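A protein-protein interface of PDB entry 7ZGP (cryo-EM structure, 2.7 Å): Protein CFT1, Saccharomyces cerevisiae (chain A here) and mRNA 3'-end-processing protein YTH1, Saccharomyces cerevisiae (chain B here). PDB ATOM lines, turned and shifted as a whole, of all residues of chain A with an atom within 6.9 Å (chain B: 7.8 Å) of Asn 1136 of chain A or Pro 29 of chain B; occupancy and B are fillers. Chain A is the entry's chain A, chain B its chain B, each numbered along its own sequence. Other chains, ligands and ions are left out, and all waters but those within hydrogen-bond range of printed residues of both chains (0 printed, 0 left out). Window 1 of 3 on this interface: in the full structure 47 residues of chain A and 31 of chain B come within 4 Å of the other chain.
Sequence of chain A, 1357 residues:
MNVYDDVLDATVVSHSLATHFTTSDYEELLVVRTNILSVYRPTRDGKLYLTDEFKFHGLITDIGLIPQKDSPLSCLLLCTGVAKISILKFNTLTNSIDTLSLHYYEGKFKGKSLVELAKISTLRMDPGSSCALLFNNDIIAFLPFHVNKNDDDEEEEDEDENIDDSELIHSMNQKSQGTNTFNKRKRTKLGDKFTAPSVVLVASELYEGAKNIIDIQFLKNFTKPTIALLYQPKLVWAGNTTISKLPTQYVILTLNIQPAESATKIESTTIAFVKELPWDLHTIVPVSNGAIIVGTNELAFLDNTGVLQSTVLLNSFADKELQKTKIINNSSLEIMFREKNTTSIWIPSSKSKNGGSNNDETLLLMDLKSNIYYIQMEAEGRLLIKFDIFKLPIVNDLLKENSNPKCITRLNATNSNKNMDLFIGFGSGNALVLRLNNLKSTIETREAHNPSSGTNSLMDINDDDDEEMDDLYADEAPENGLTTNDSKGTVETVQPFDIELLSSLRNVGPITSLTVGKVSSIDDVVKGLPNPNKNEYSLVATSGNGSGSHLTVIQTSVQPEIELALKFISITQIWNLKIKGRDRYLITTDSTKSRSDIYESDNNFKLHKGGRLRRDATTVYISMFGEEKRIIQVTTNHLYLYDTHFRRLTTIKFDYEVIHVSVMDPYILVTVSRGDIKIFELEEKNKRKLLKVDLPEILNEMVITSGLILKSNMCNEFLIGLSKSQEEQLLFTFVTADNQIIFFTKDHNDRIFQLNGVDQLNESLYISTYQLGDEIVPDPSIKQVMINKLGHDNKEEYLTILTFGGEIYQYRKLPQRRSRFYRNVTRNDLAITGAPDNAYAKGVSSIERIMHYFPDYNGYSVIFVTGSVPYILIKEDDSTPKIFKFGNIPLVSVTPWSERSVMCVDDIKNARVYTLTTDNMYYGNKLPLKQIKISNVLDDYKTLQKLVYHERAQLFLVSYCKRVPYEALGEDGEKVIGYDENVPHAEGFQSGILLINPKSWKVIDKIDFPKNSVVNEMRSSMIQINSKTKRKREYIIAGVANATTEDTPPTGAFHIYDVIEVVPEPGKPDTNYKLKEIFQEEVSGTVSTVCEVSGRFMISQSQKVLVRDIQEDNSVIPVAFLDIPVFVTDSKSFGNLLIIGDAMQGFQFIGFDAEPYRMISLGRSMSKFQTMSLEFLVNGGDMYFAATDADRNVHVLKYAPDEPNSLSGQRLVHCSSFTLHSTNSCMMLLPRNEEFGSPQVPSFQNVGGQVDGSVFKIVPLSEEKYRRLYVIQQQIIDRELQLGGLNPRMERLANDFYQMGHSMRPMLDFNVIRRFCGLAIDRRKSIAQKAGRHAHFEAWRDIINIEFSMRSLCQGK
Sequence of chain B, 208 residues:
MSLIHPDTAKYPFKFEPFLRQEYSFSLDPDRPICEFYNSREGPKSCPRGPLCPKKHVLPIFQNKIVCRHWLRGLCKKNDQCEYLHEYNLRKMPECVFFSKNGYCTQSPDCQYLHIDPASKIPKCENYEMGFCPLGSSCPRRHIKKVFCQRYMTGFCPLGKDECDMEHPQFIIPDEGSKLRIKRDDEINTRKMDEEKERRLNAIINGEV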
ATOM      1  N   VAL A1093     -31.346 -19.003   6.050  1.00  0.00           N
ATOM      2  CA  VAL A1093     -29.910 -19.179   5.882  1.00  0.00           C
ATOM      3  C   VAL A1093     -29.355 -19.902   7.104  1.00  0.00           C
ATOM      4  O   VAL A1093     -29.454 -19.402   8.230  1.00  0.00           O
ATOM      5  CB  VAL A1093     -29.190 -17.840   5.637  1.00  0.00           C
ATOM      6  CG1 VAL A1093     -29.417 -16.857   6.778  1.00  0.00           C
ATOM      7  CG2 VAL A1093     -27.712 -18.089   5.458  1.00  0.00           C
ATOM      8  N   SER A1094     -28.799 -21.094   6.879  1.00  0.00           N
ATOM      9  CA  SER A1094     -28.099 -21.862   7.910  1.00  0.00           C
ATOM     10  C   SER A1094     -28.926 -21.990   9.187  1.00  0.00           C
ATOM     11  O   SER A1094     -28.432 -21.782  10.296  1.00  0.00           O
ATOM     12  CB  SER A1094     -26.733 -21.247   8.208  1.00  0.00           C
ATOM     13  OG  SER A1094     -26.866 -20.046   8.944  1.00  0.00           O
ATOM     14  N   ARG A1096     -31.333 -20.089  10.170  1.00  0.00           N
ATOM     15  CA  ARG A1096     -31.917 -18.815  10.554  1.00  0.00           C
ATOM     16  C   ARG A1096     -32.562 -18.191   9.328  1.00  0.00           C
ATOM     17  O   ARG A1096     -32.125 -18.421   8.198  1.00  0.00           O
ATOM     18  CB  ARG A1096     -30.861 -17.875  11.142  1.00  0.00           C
ATOM     19  CG  ARG A1096     -30.116 -18.466  12.324  1.00  0.00           C
ATOM     20  CD  ARG A1096     -28.760 -17.816  12.508  1.00  0.00           C
ATOM     21  NE  ARG A1096     -27.959 -18.500  13.514  1.00  0.00           N
ATOM     22  CZ  ARG A1096     -27.177 -19.542  13.266  1.00  0.00           C
ATOM     23  NH1 ARG A1096     -27.077 -20.056  12.052  1.00  0.00           N
ATOM     24  NH2 ARG A1096     -26.478 -20.079  14.260  1.00  0.00           N
ATOM     25  N   SER A1133     -30.799 -18.914  -0.649  1.00  0.00           N
ATOM     26  CA  SER A1133     -29.657 -19.250   0.186  1.00  0.00           C
ATOM     27  C   SER A1133     -29.141 -20.632  -0.174  1.00  0.00           C
ATOM     28  O   SER A1133     -29.922 -21.539  -0.473  1.00  0.00           O
ATOM     29  CB  SER A1133     -30.020 -19.200   1.671  1.00  0.00           C
ATOM     30  OG  SER A1133     -30.902 -20.253   2.016  1.00  0.00           O
ATOM     31  N   PHE A1134     -27.815 -20.788  -0.146  1.00  0.00           N
ATOM     32  CA  PHE A1134     -27.149 -22.066  -0.404  1.00  0.00           C
ATOM     33  C   PHE A1134     -26.246 -22.359   0.792  1.00  0.00           C
ATOM     34  O   PHE A1134     -25.053 -22.050   0.780  1.00  0.00           O
ATOM     35  CB  PHE A1134     -26.372 -22.025  -1.712  1.00  0.00           C
ATOM     36  CG  PHE A1134     -26.019 -23.381  -2.245  1.00  0.00           C
ATOM     37  CD1 PHE A1134     -24.880 -24.036  -1.812  1.00  0.00           C
ATOM     38  CD2 PHE A1134     -26.829 -24.003  -3.177  1.00  0.00           C
ATOM     39  CE1 PHE A1134     -24.556 -25.283  -2.299  1.00  0.00           C
ATOM     40  CE2 PHE A1134     -26.511 -25.249  -3.666  1.00  0.00           C
ATOM     41  CZ  PHE A1134     -25.371 -25.890  -3.227  1.00  0.00           C
ATOM     42  N   GLY A1135     -26.827 -22.955   1.826  1.00  0.00           N
ATOM     43  CA  GLY A1135     -26.093 -23.279   3.033  1.00  0.00           C
ATOM     44  C   GLY A1135     -25.936 -22.073   3.933  1.00  0.00           C
ATOM     45  O   GLY A1135     -26.650 -21.934   4.930  1.00  0.00           O
ATOM     46  N   ASN A1136     -25.001 -21.185   3.585  1.00  0.00           N
ATOM     47  CA  ASN A1136     -24.898 -19.901   4.265  1.00  0.00           C
ATOM     48  C   ASN A1136     -24.530 -18.777   3.303  1.00  0.00           C
ATOM     49  O   ASN A1136     -23.972 -17.763   3.734  1.00  0.00           O
ATOM     50  CB  ASN A1136     -23.890 -19.958   5.416  1.00  0.00           C
ATOM     51  CG  ASN A1136     -22.477 -20.224   4.948  1.00  0.00           C
ATOM     52  OD1 ASN A1136     -22.257 -20.711   3.841  1.00  0.00           O
ATOM     53  ND2 ASN A1136     -21.507 -19.906   5.794  1.00  0.00           N
ATOM     54  N   LEU A1137     -24.836 -18.927   2.019  1.00  0.00           N
ATOM     55  CA  LEU A1137     -24.525 -17.930   1.005  1.00  0.00           C
ATOM     56  C   LEU A1137     -25.828 -17.378   0.449  1.00  0.00           C
ATOM     57  O   LEU A1137     -26.674 -18.140  -0.025  1.00  0.00           O
ATOM     58  CB  LEU A1137     -23.673 -18.539  -0.106  1.00  0.00           C
ATOM     59  CG  LEU A1137     -22.378 -19.203   0.364  1.00  0.00           C
ATOM     60  CD1 LEU A1137     -21.676 -19.892  -0.791  1.00  0.00           C
ATOM     61  CD2 LEU A1137     -21.466 -18.182   1.019  1.00  0.00           C
ATOM     62  N   LEU A1138     -25.983 -16.059   0.499  1.00  0.00           N
ATOM     63  CA  LEU A1138     -27.206 -15.400   0.066  1.00  0.00           C
ATOM     64  C   LEU A1138     -27.020 -14.764  -1.302  1.00  0.00           C
ATOM     65  O   LEU A1138     -25.927 -14.316  -1.657  1.00  0.00           O
ATOM     66  CB  LEU A1138     -27.634 -14.313   1.056  1.00  0.00           C
ATOM     67  CG  LEU A1138     -28.357 -14.687   2.347  1.00  0.00           C
ATOM     68  CD1 LEU A1138     -29.547 -15.587   2.060  1.00  0.00           C
ATOM     69  CD2 LEU A1138     -27.401 -15.321   3.332  1.00  0.00           C
ATOM     70  N   PHE A1149     -24.192 -10.916  -3.849  1.00  0.00           N
ATOM     71  CA  PHE A1149     -23.837 -12.202  -3.264  1.00  0.00           C
ATOM     72  C   PHE A1149     -23.353 -11.962  -1.840  1.00  0.00           C
ATOM     73  O   PHE A1149     -22.414 -11.189  -1.627  1.00  0.00           O
ATOM     74  CB  PHE A1149     -22.762 -12.883  -4.112  1.00  0.00           C
ATOM     75  CG  PHE A1149     -22.380 -14.256  -3.643  1.00  0.00           C
ATOM     76  CD1 PHE A1149     -23.324 -15.113  -3.113  1.00  0.00           C
ATOM     77  CD2 PHE A1149     -21.073 -14.696  -3.757  1.00  0.00           C
ATOM     78  CE1 PHE A1149     -22.971 -16.375  -2.693  1.00  0.00           C
ATOM     79  CE2 PHE A1149     -20.714 -15.957  -3.339  1.00  0.00           C
ATOM     80  CZ  PHE A1149     -21.664 -16.799  -2.805  1.00  0.00           C
ATOM     81  N   ILE A1150     -23.993 -12.614  -0.873  1.00  0.00           N
ATOM     82  CA  ILE A1150     -23.731 -12.376   0.542  1.00  0.00           C
ATOM     83  C   ILE A1150     -23.431 -13.697   1.231  1.00  0.00           C
ATOM     84  O   ILE A1150     -24.133 -14.691   1.023  1.00  0.00           O
ATOM     85  CB  ILE A1150     -24.919 -11.673   1.234  1.00  0.00           C
ATOM     86  CG1 ILE A1150     -25.048 -10.232   0.753  1.00  0.00           C
ATOM     87  CG2 ILE A1150     -24.769 -11.708   2.742  1.00  0.00           C
ATOM     88  CD1 ILE A1150     -26.076 -10.062  -0.316  1.00  0.00           C
ATOM     89  N   GLY A1151     -22.385 -13.705   2.051  1.00  0.00           N
ATOM     90  CA  GLY A1151     -22.108 -14.813   2.948  1.00  0.00           C
ATOM     91  C   GLY A1151     -22.558 -14.468   4.358  1.00  0.00           C
ATOM     92  O   GLY A1151     -22.418 -13.330   4.804  1.00  0.00           O
ATOM     93  N   PHE A1152     -23.103 -15.462   5.052  1.00  0.00           N
ATOM     94  CA  PHE A1152     -23.627 -15.284   6.398  1.00  0.00           C
ATOM     95  C   PHE A1152     -22.774 -16.063   7.389  1.00  0.00           C
ATOM     96  O   PHE A1152     -22.475 -17.240   7.167  1.00  0.00           O
ATOM     97  CB  PHE A1152     -25.086 -15.739   6.485  1.00  0.00           C
ATOM     98  CG  PHE A1152     -25.623 -15.782   7.885  1.00  0.00           C
ATOM     99  CD1 PHE A1152     -25.946 -14.614   8.552  1.00  0.00           C
ATOM    100  CD2 PHE A1152     -25.801 -16.990   8.537  1.00  0.00           C
ATOM    101  CE1 PHE A1152     -26.437 -14.650   9.839  1.00  0.00           C
ATOM    102  CE2 PHE A1152     -26.292 -17.030   9.825  1.00  0.00           C
ATOM    103  CZ  PHE A1152     -26.610 -15.858  10.476  1.00  0.00           C
ATOM    104  N   ASP A1153     -22.384 -15.405   8.488  1.00  0.00           N
ATOM    105  CA  ASP A1153     -21.587 -16.075   9.553  1.00  0.00           C
ATOM    106  C   ASP A1153     -22.402 -16.050  10.851  1.00  0.00           C
ATOM    107  O   ASP A1153     -23.407 -15.320  10.884  1.00  0.00           O
ATOM    108  CB  ASP A1153     -20.206 -15.435   9.704  1.00  0.00           C
ATOM    109  CG  ASP A1153     -19.210 -16.309  10.445  1.00  0.00           C
ATOM    110  OD1 ASP A1153     -19.513 -17.502  10.643  1.00  0.00           O
ATOM    111  OD2 ASP A1153     -18.142 -15.788  10.821  1.00  0.00           O
ATOM    112  N   ALA A1154     -21.988 -16.793  11.883  1.00  0.00           N
ATOM    113  CA  ALA A1154     -22.826 -16.892  13.104  1.00  0.00           C
ATOM    114  C   ALA A1154     -22.169 -16.233  14.324  1.00  0.00           C
ATOM    115  O   ALA A1154     -22.399 -15.031  14.511  1.00  0.00           O
ATOM    116  CB  ALA A1154     -23.153 -18.339  13.377  1.00  0.00           C
ATOM    117  N   GLU A1155     -21.409 -16.984  15.132  1.00  0.00           N
ATOM    118  CA  GLU A1155     -20.853 -16.428  16.404  1.00  0.00           C
ATOM    119  C   GLU A1155     -20.755 -14.906  16.284  1.00  0.00           C
ATOM    120  O   GLU A1155     -21.563 -14.224  16.941  1.00  0.00           O
ATOM    121  CB  GLU A1155     -19.484 -17.035  16.713  1.00  0.00           C
ATOM    122  N   PRO A1156     -19.822 -14.328  15.496  1.00  0.00           N
ATOM    123  CA  PRO A1156     -19.801 -12.890  15.275  1.00  0.00           C
ATOM    124  C   PRO A1156     -20.712 -12.698  14.059  1.00  0.00           C
ATOM    125  O   PRO A1156     -20.211 -12.710  12.956  1.00  0.00           O
ATOM    126  CB  PRO A1156     -18.325 -12.614  14.977  1.00  0.00           C
ATOM    127  CG  PRO A1156     -17.824 -13.883  14.313  1.00  0.00           C
ATOM    128  CD  PRO A1156     -18.752 -14.998  14.755  1.00  0.00           C
ATOM    129  N   LEU A1162     -19.908 -10.564  -0.499  1.00  0.00           N
ATOM    130  CA  LEU A1162     -18.949 -11.323  -1.291  1.00  0.00           C
ATOM    131  C   LEU A1162     -18.839 -10.792  -2.713  1.00  0.00           C
ATOM    132  O   LEU A1162     -17.767 -10.874  -3.322  1.00  0.00           O
ATOM    133  CB  LEU A1162     -19.335 -12.800  -1.301  1.00  0.00           C
ATOM    134  CG  LEU A1162     -19.305 -13.485   0.065  1.00  0.00           C
ATOM    135  CD1 LEU A1162     -19.845 -14.898  -0.031  1.00  0.00           C
ATOM    136  CD2 LEU A1162     -17.895 -13.486   0.622  1.00  0.00           C
ATOM    137  N   THR B   8     -27.655 -28.337   1.094  1.00  0.00           N
ATOM    138  CA  THR B   8     -26.708 -27.416   0.481  1.00  0.00           C
ATOM    139  C   THR B   8     -25.716 -26.846   1.487  1.00  0.00           C
ATOM    140  O   THR B   8     -24.987 -25.906   1.159  1.00  0.00           O
ATOM    141  CB  THR B   8     -27.457 -26.278  -0.216  1.00  0.00           C
ATOM    142  OG1 THR B   8     -28.173 -25.512   0.759  1.00  0.00           O
ATOM    143  CG2 THR B   8     -28.447 -26.836  -1.224  1.00  0.00           C
ATOM    144  N   ALA B   9     -25.669 -27.392   2.702  1.00  0.00           N
ATOM    145  CA  ALA B   9     -24.845 -26.802   3.752  1.00  0.00           C
ATOM    146  C   ALA B   9     -23.363 -27.062   3.510  1.00  0.00           C
ATOM    147  O   ALA B   9     -22.577 -26.126   3.326  1.00  0.00           O
ATOM    148  CB  ALA B   9     -25.274 -27.344   5.117  1.00  0.00           C
ATOM    149  N   LYS B  10     -22.959 -28.332   3.505  1.00  0.00           N
ATOM    150  CA  LYS B  10     -21.551 -28.703   3.370  1.00  0.00           C
ATOM    151  C   LYS B  10     -21.272 -29.040   1.908  1.00  0.00           C
ATOM    152  O   LYS B  10     -21.162 -30.201   1.515  1.00  0.00           O
ATOM    153  CB  LYS B  10     -21.209 -29.867   4.294  1.00  0.00           C
ATOM    154  CG  LYS B  10     -21.863 -29.785   5.661  1.00  0.00           C
ATOM    155  CD  LYS B  10     -21.286 -28.641   6.478  1.00  0.00           C
ATOM    156  CE  LYS B  10     -19.954 -29.028   7.098  1.00  0.00           C
ATOM    157  NZ  LYS B  10     -19.455 -27.982   8.031  1.00  0.00           N
ATOM    158  N   PHE B  13     -16.675 -26.274  -2.269  1.00  0.00           N
ATOM    159  CA  PHE B  13     -16.483 -25.143  -3.162  1.00  0.00           C
ATOM    160  C   PHE B  13     -14.996 -24.878  -3.347  1.00  0.00           C
ATOM    161  O   PHE B  13     -14.206 -25.041  -2.412  1.00  0.00           O
ATOM    162  CB  PHE B  13     -17.180 -23.895  -2.618  1.00  0.00           C
ATOM    163  CG  PHE B  13     -18.647 -23.836  -2.929  1.00  0.00           C
ATOM    164  CD1 PHE B  13     -19.093 -23.845  -4.239  1.00  0.00           C
ATOM    165  CD2 PHE B  13     -19.582 -23.778  -1.910  1.00  0.00           C
ATOM    166  CE1 PHE B  13     -20.440 -23.792  -4.527  1.00  0.00           C
ATOM    167  CE2 PHE B  13     -20.932 -23.725  -2.192  1.00  0.00           C
ATOM    168  CZ  PHE B  13     -21.360 -23.733  -3.502  1.00  0.00           C
ATOM    169  N   GLU B  16     -13.515 -21.869  -1.184  1.00  0.00           N
ATOM    170  CA  GLU B  16     -13.550 -21.939   0.276  1.00  0.00           C
ATOM    171  C   GLU B  16     -12.228 -21.532   0.915  1.00  0.00           C
ATOM    172  O   GLU B  16     -12.255 -20.775   1.902  1.00  0.00           O
ATOM    173  CB  GLU B  16     -13.985 -23.344   0.709  1.00  0.00           C
ATOM    174  CG  GLU B  16     -13.567 -23.743   2.118  1.00  0.00           C
ATOM    175  CD  GLU B  16     -14.429 -23.104   3.194  1.00  0.00           C
ATOM    176  OE1 GLU B  16     -14.458 -21.859   3.288  1.00  0.00           O
ATOM    177  OE2 GLU B  16     -15.081 -23.852   3.951  1.00  0.00           O
ATOM    178  N   LEU B  19     -12.238 -17.868   0.862  1.00  0.00           N
ATOM    179  CA  LEU B  19     -13.122 -17.343   1.896  1.00  0.00           C
ATOM    180  C   LEU B  19     -12.498 -17.460   3.278  1.00  0.00           C
ATOM    181  O   LEU B  19     -12.854 -16.700   4.182  1.00  0.00           O
ATOM    182  CB  LEU B  19     -14.466 -18.068   1.858  1.00  0.00           C
ATOM    183  CG  LEU B  19     -15.337 -17.815   0.627  1.00  0.00           C
ATOM    184  CD1 LEU B  19     -16.710 -18.431   0.814  1.00  0.00           C
ATOM    185  CD2 LEU B  19     -15.450 -16.329   0.343  1.00  0.00           C
ATOM    186  N   PHE B  25     -13.869 -16.147   6.507  1.00  0.00           N
ATOM    187  CA  PHE B  25     -15.181 -16.752   6.352  1.00  0.00           C
ATOM    188  C   PHE B  25     -15.044 -18.237   6.036  1.00  0.00           C
ATOM    189  O   PHE B  25     -13.969 -18.722   5.676  1.00  0.00           O
ATOM    190  CB  PHE B  25     -15.962 -16.038   5.240  1.00  0.00           C
ATOM    191  CG  PHE B  25     -17.413 -16.407   5.171  1.00  0.00           C
ATOM    192  CD1 PHE B  25     -18.184 -16.468   6.317  1.00  0.00           C
ATOM    193  CD2 PHE B  25     -18.010 -16.685   3.955  1.00  0.00           C
ATOM    194  CE1 PHE B  25     -19.518 -16.804   6.252  1.00  0.00           C
ATOM    195  CE2 PHE B  25     -19.343 -17.022   3.883  1.00  0.00           C
ATOM    196  CZ  PHE B  25     -20.098 -17.081   5.033  1.00  0.00           C
ATOM    197  N   SER B  26     -16.147 -18.962   6.191  1.00  0.00           N
ATOM    198  CA  SER B  26     -16.205 -20.365   5.809  1.00  0.00           C
ATOM    199  C   SER B  26     -17.647 -20.712   5.467  1.00  0.00           C
ATOM    200  O   SER B  26     -18.535 -19.857   5.491  1.00  0.00           O
ATOM    201  CB  SER B  26     -15.664 -21.270   6.920  1.00  0.00           C
ATOM    202  OG  SER B  26     -16.682 -21.595   7.849  1.00  0.00           O
ATOM    203  N   LEU B  27     -17.877 -21.983   5.150  1.00  0.00           N
ATOM    204  CA  LEU B  27     -19.210 -22.467   4.821  1.00  0.00           C
ATOM    205  C   LEU B  27     -19.914 -23.122   6.002  1.00  0.00           C
ATOM    206  O   LEU B  27     -21.012 -23.658   5.826  1.00  0.00           O
ATOM    207  CB  LEU B  27     -19.138 -23.446   3.648  1.00  0.00           C
ATOM    208  CG  LEU B  27     -18.401 -22.907   2.423  1.00  0.00           C
ATOM    209  CD1 LEU B  27     -18.120 -24.018   1.428  1.00  0.00           C
ATOM    210  CD2 LEU B  27     -19.197 -21.788   1.774  1.00  0.00           C
ATOM    211  N   ASP B  28     -19.317 -23.092   7.193  1.00  0.00           N
ATOM    212  CA  ASP B  28     -19.930 -23.634   8.404  1.00  0.00           C
ATOM    213  C   ASP B  28     -20.108 -22.487   9.389  1.00  0.00           C
ATOM    214  O   ASP B  28     -19.175 -22.150  10.133  1.00  0.00           O
ATOM    215  CB  ASP B  28     -19.063 -24.743   9.005  1.00  0.00           C
ATOM    216  CG  ASP B  28     -19.684 -25.376  10.242  1.00  0.00           C
ATOM    217  OD1 ASP B  28     -20.803 -24.984  10.634  1.00  0.00           O
ATOM    218  OD2 ASP B  28     -19.056 -26.293  10.811  1.00  0.00           O
ATOM    219  N   PRO B  29     -21.279 -21.843   9.426  1.00  0.00           N
ATOM    220  CA  PRO B  29     -21.457 -20.707  10.347  1.00  0.00           C
ATOM    221  C   PRO B  29     -21.261 -21.074  11.806  1.00  0.00           C
ATOM    222  O   PRO B  29     -20.688 -20.287  12.567  1.00  0.00           O
ATOM    223  CB  PRO B  29     -22.897 -20.250  10.068  1.00  0.00           C
ATOM    224  CG  PRO B  29     -23.247 -20.840   8.752  1.00  0.00           C
ATOM    225  CD  PRO B  29     -22.495 -22.122   8.649  1.00  0.00           C
ATOM    226  N   ASP B  30     -21.721 -22.250  12.217  1.00  0.00           N
ATOM    227  CA  ASP B  30     -21.554 -22.701  13.599  1.00  0.00           C
ATOM    228  C   ASP B  30     -20.301 -23.555  13.761  1.00  0.00           C
ATOM    229  O   ASP B  30     -20.344 -24.666  14.284  1.00  0.00           O
ATOM    230  CB  ASP B  30     -22.798 -23.457  14.051  1.00  0.00           C
ATOM    231  CG  ASP B  30     -24.082 -22.738  13.684  1.00  0.00           C
ATOM    232  OD1 ASP B  30     -24.440 -21.768  14.384  1.00  0.00           O
ATOM    233  OD2 ASP B  30     -24.731 -23.139  12.697  1.00  0.00           O
ATOM    234  N   ARG B  31     -19.165 -23.029  13.311  1.00  0.00           N
ATOM    235  CA  ARG B  31     -17.949 -23.789  13.542  1.00  0.00           C
ATOM    236  C   ARG B  31     -17.337 -23.411  14.888  1.00  0.00           C
ATOM    237  O   ARG B  31     -17.499 -22.280  15.355  1.00  0.00           O
ATOM    238  CB  ARG B  31     -16.942 -23.540  12.420  1.00  0.00           C
ATOM    239  CG  ARG B  31     -16.450 -22.110  12.305  1.00  0.00           C
ATOM    240  CD  ARG B  31     -15.882 -21.854  10.921  1.00  0.00           C
ATOM    241  NE  ARG B  31     -15.490 -20.465  10.719  1.00  0.00           N
ATOM    242  CZ  ARG B  31     -16.333 -19.479  10.446  1.00  0.00           C
ATOM    243  NH1 ARG B  31     -17.634 -19.692  10.342  1.00  0.00           N
ATOM    244  NH2 ARG B  31     -15.859 -18.250  10.266  1.00  0.00           N
ATOM    245  N   PRO B  32     -16.641 -24.344  15.538  1.00  0.00           N
ATOM    246  CA  PRO B  32     -16.091 -24.055  16.867  1.00  0.00           C
ATOM    247  C   PRO B  32     -15.044 -22.954  16.814  1.00  0.00           C
ATOM    248  O   PRO B  32     -14.357 -22.763  15.808  1.00  0.00           O
ATOM    249  CB  PRO B  32     -15.478 -25.392  17.300  1.00  0.00           C
ATOM    250  CG  PRO B  32     -15.294 -26.164  16.039  1.00  0.00           C
ATOM    251  CD  PRO B  32     -16.386 -25.732  15.120  1.00  0.00           C
ATOM    252  N   LYS B  55     -12.800 -20.752  13.946  1.00  0.00           N
ATOM    253  CA  LYS B  55     -13.242 -19.351  13.726  1.00  0.00           C
ATOM    254  C   LYS B  55     -12.224 -18.366  14.299  1.00  0.00           C
ATOM    255  O   LYS B  55     -11.882 -18.495  15.488  1.00  0.00           O
ATOM    256  CB  LYS B  55     -14.627 -19.131  14.344  1.00  0.00           C
ATOM    257  CG  LYS B  55     -15.236 -17.760  14.091  1.00  0.00           C
ATOM    258  CD  LYS B  55     -16.725 -17.703  14.354  1.00  0.00           C
ATOM    259  CE  LYS B  55     -17.528 -18.576  13.412  1.00  0.00           C
ATOM    260  NZ  LYS B  55     -18.982 -18.311  13.517  1.00  0.00           N
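The backbone carbonyl oxygen (O) of Ser 1094 of chain A sits at hydrogen-bond distance from the guanidinium group (NH1) of Arg 1096 of chain A, at 2.8 Å.
The side-chain hydroxyl (OG) of Ser 26 of chain B lies within hydrogen-bond range of the backbone NH (N) of Asp 28 of chain B, 3.1 Å away.
The backbone NH of Lys 55 of chain B is in hydrogen-bond range of the backbone carbonyl oxygen of Pro 32 of chain B, 3.2 Å away.
Among the printed residues, merely in contact across the chains: Phe 1152 of chain A with Phe 25 of chain B (3.1 Å), Ala 1154 of chain A with Pro 29 of chain B (3.2 Å), Asn 1136 of chain A with Phe 25 of chain B (3.2 Å), Pro 1156 of chain A with Lys 55 of chain B (3.4 Å), Phe 1134 of chain A with Thr 8 of chain B (3.5 Å), Asn 1136 of chain A with Pro 29 of chain B (3.5 Å), Ser 1094 of chain A with Pro 29 of chain B (3.6 Å), Asn 1136 of chain A with Leu 27 of chain B (3.6 Å), Asp 1153 of chain A with Pro 29 of chain B (3.6 Å), Gly 1151 of chain A with Phe 25 of chain B (3.7 Å), Ala 1154 of chain A with Lys 55 of chain B (3.7 Å), Leu 1137 of chain A with Phe 25 of chain B (3.7 Å), Phe 1134 of chain A with Phe 13 of chain B (3.8 Å), Leu 1162 of chain A with Leu 19 of chain B (3.8 Å), Asp 1153 of chain A with Phe 25 of chain B (3.8 Å), Ala 1154 of chain A with Asp 30 of chain B (3.8 Å) and Gly 1135 of chain A with Ala 9 of chain B (3.8 Å).
Of the 18 printed residues of chain A, 13 touch a printed residue of chain B.
Hydrophobic or aromatic side chains of chain A that line the printed part of chain B: Phe 1134, Leu 1137, Ala 1154, Pro 1156 and Leu 1162.
Of the 15 printed residues of chain B, 11 touch a printed residue of chain A.
Printed residues of chain B that touch a printed residue of chain A: Thr 8, Ala 9, Phe 13, Leu 19, Phe 25, Ser 26, Leu 27, Pro 29, Asp 30, Arg 31 and Lys 55.
Hydrophobic or aromatic side chains of chain B that line the printed part of chain A: Phe 13, Leu 19, Phe 25, Leu 27 and Pro 29.
Among the printed residues, 23 pairs touch across the chains.
The guanidinium group of Arg 1096 of chain A is in salt-bridge range of the side-chain carboxylate of Asp 30 of chain B.
The backbone NH (N) of Gly 1135 of chain A sits at hydrogen-bond distance from the side-chain hydroxyl (OG1) of Thr 8 of chain B, at 3.1 Å.
The side-chain amide nitrogen of Asn 1136 of chain A lies within hydrogen-bond range of the backbone carbonyl oxygen of Ser 26 of chain B, at 3.0 Å.
The side-chain carboxylate (OD1) of Asp 1153 of chain A lies within salt-bridge range of the guanidinium group (NH1) of Arg 31 of chain B (2.9 Å).
The side-chain carboxylate of Asp 1153 of chain A is in salt-bridge range of the side-chain amino group of Lys 55 of chain B, 3.0 Å away.
NZ of Lys 55 of chain B sits close to N of Glu 1155 of chain A, at 3.2 Å.
Printed residues of chain A within 4 Å of Pro 29 of chain B: Ser 1094 (3.6 Å), Asn 1136 (3.5 Å), Asp 1153 (3.6 Å) and Ala 1154 (3.2 Å).
Of chain B, only Thr 8 and Ala 9 come within 4 Å of Gly 1135 of chain A.
Of the printed residues of chain A, Leu 27 of chain B touches Asn 1136.
Printed residues of chain A within 4 Å of Asp 30 of chain B: Arg 1096 and Ala 1154.
Printed residues of chain A within 4 Å of Phe 13 of chain B: Phe 1134 (3.8 Å).
Printed residues of chain A within 4 Å of Leu 19 of chain B: Leu 1162 (3.8 Å).
Glu 16 of chain B touches none of the printed residues of chain A.
The nearest residue of chain B that does not touch Asn 1136 of chain A is Asp 28 of chain B (4.1 Å).
The nearest printed residue of chain A that does not touch Pro 29 of chain B is Phe 1152 of chain A (4.01 Å).
The nearest printed residue of chain B that does not touch Leu 1137 of chain A is Leu 27 of chain B (4.04 Å).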
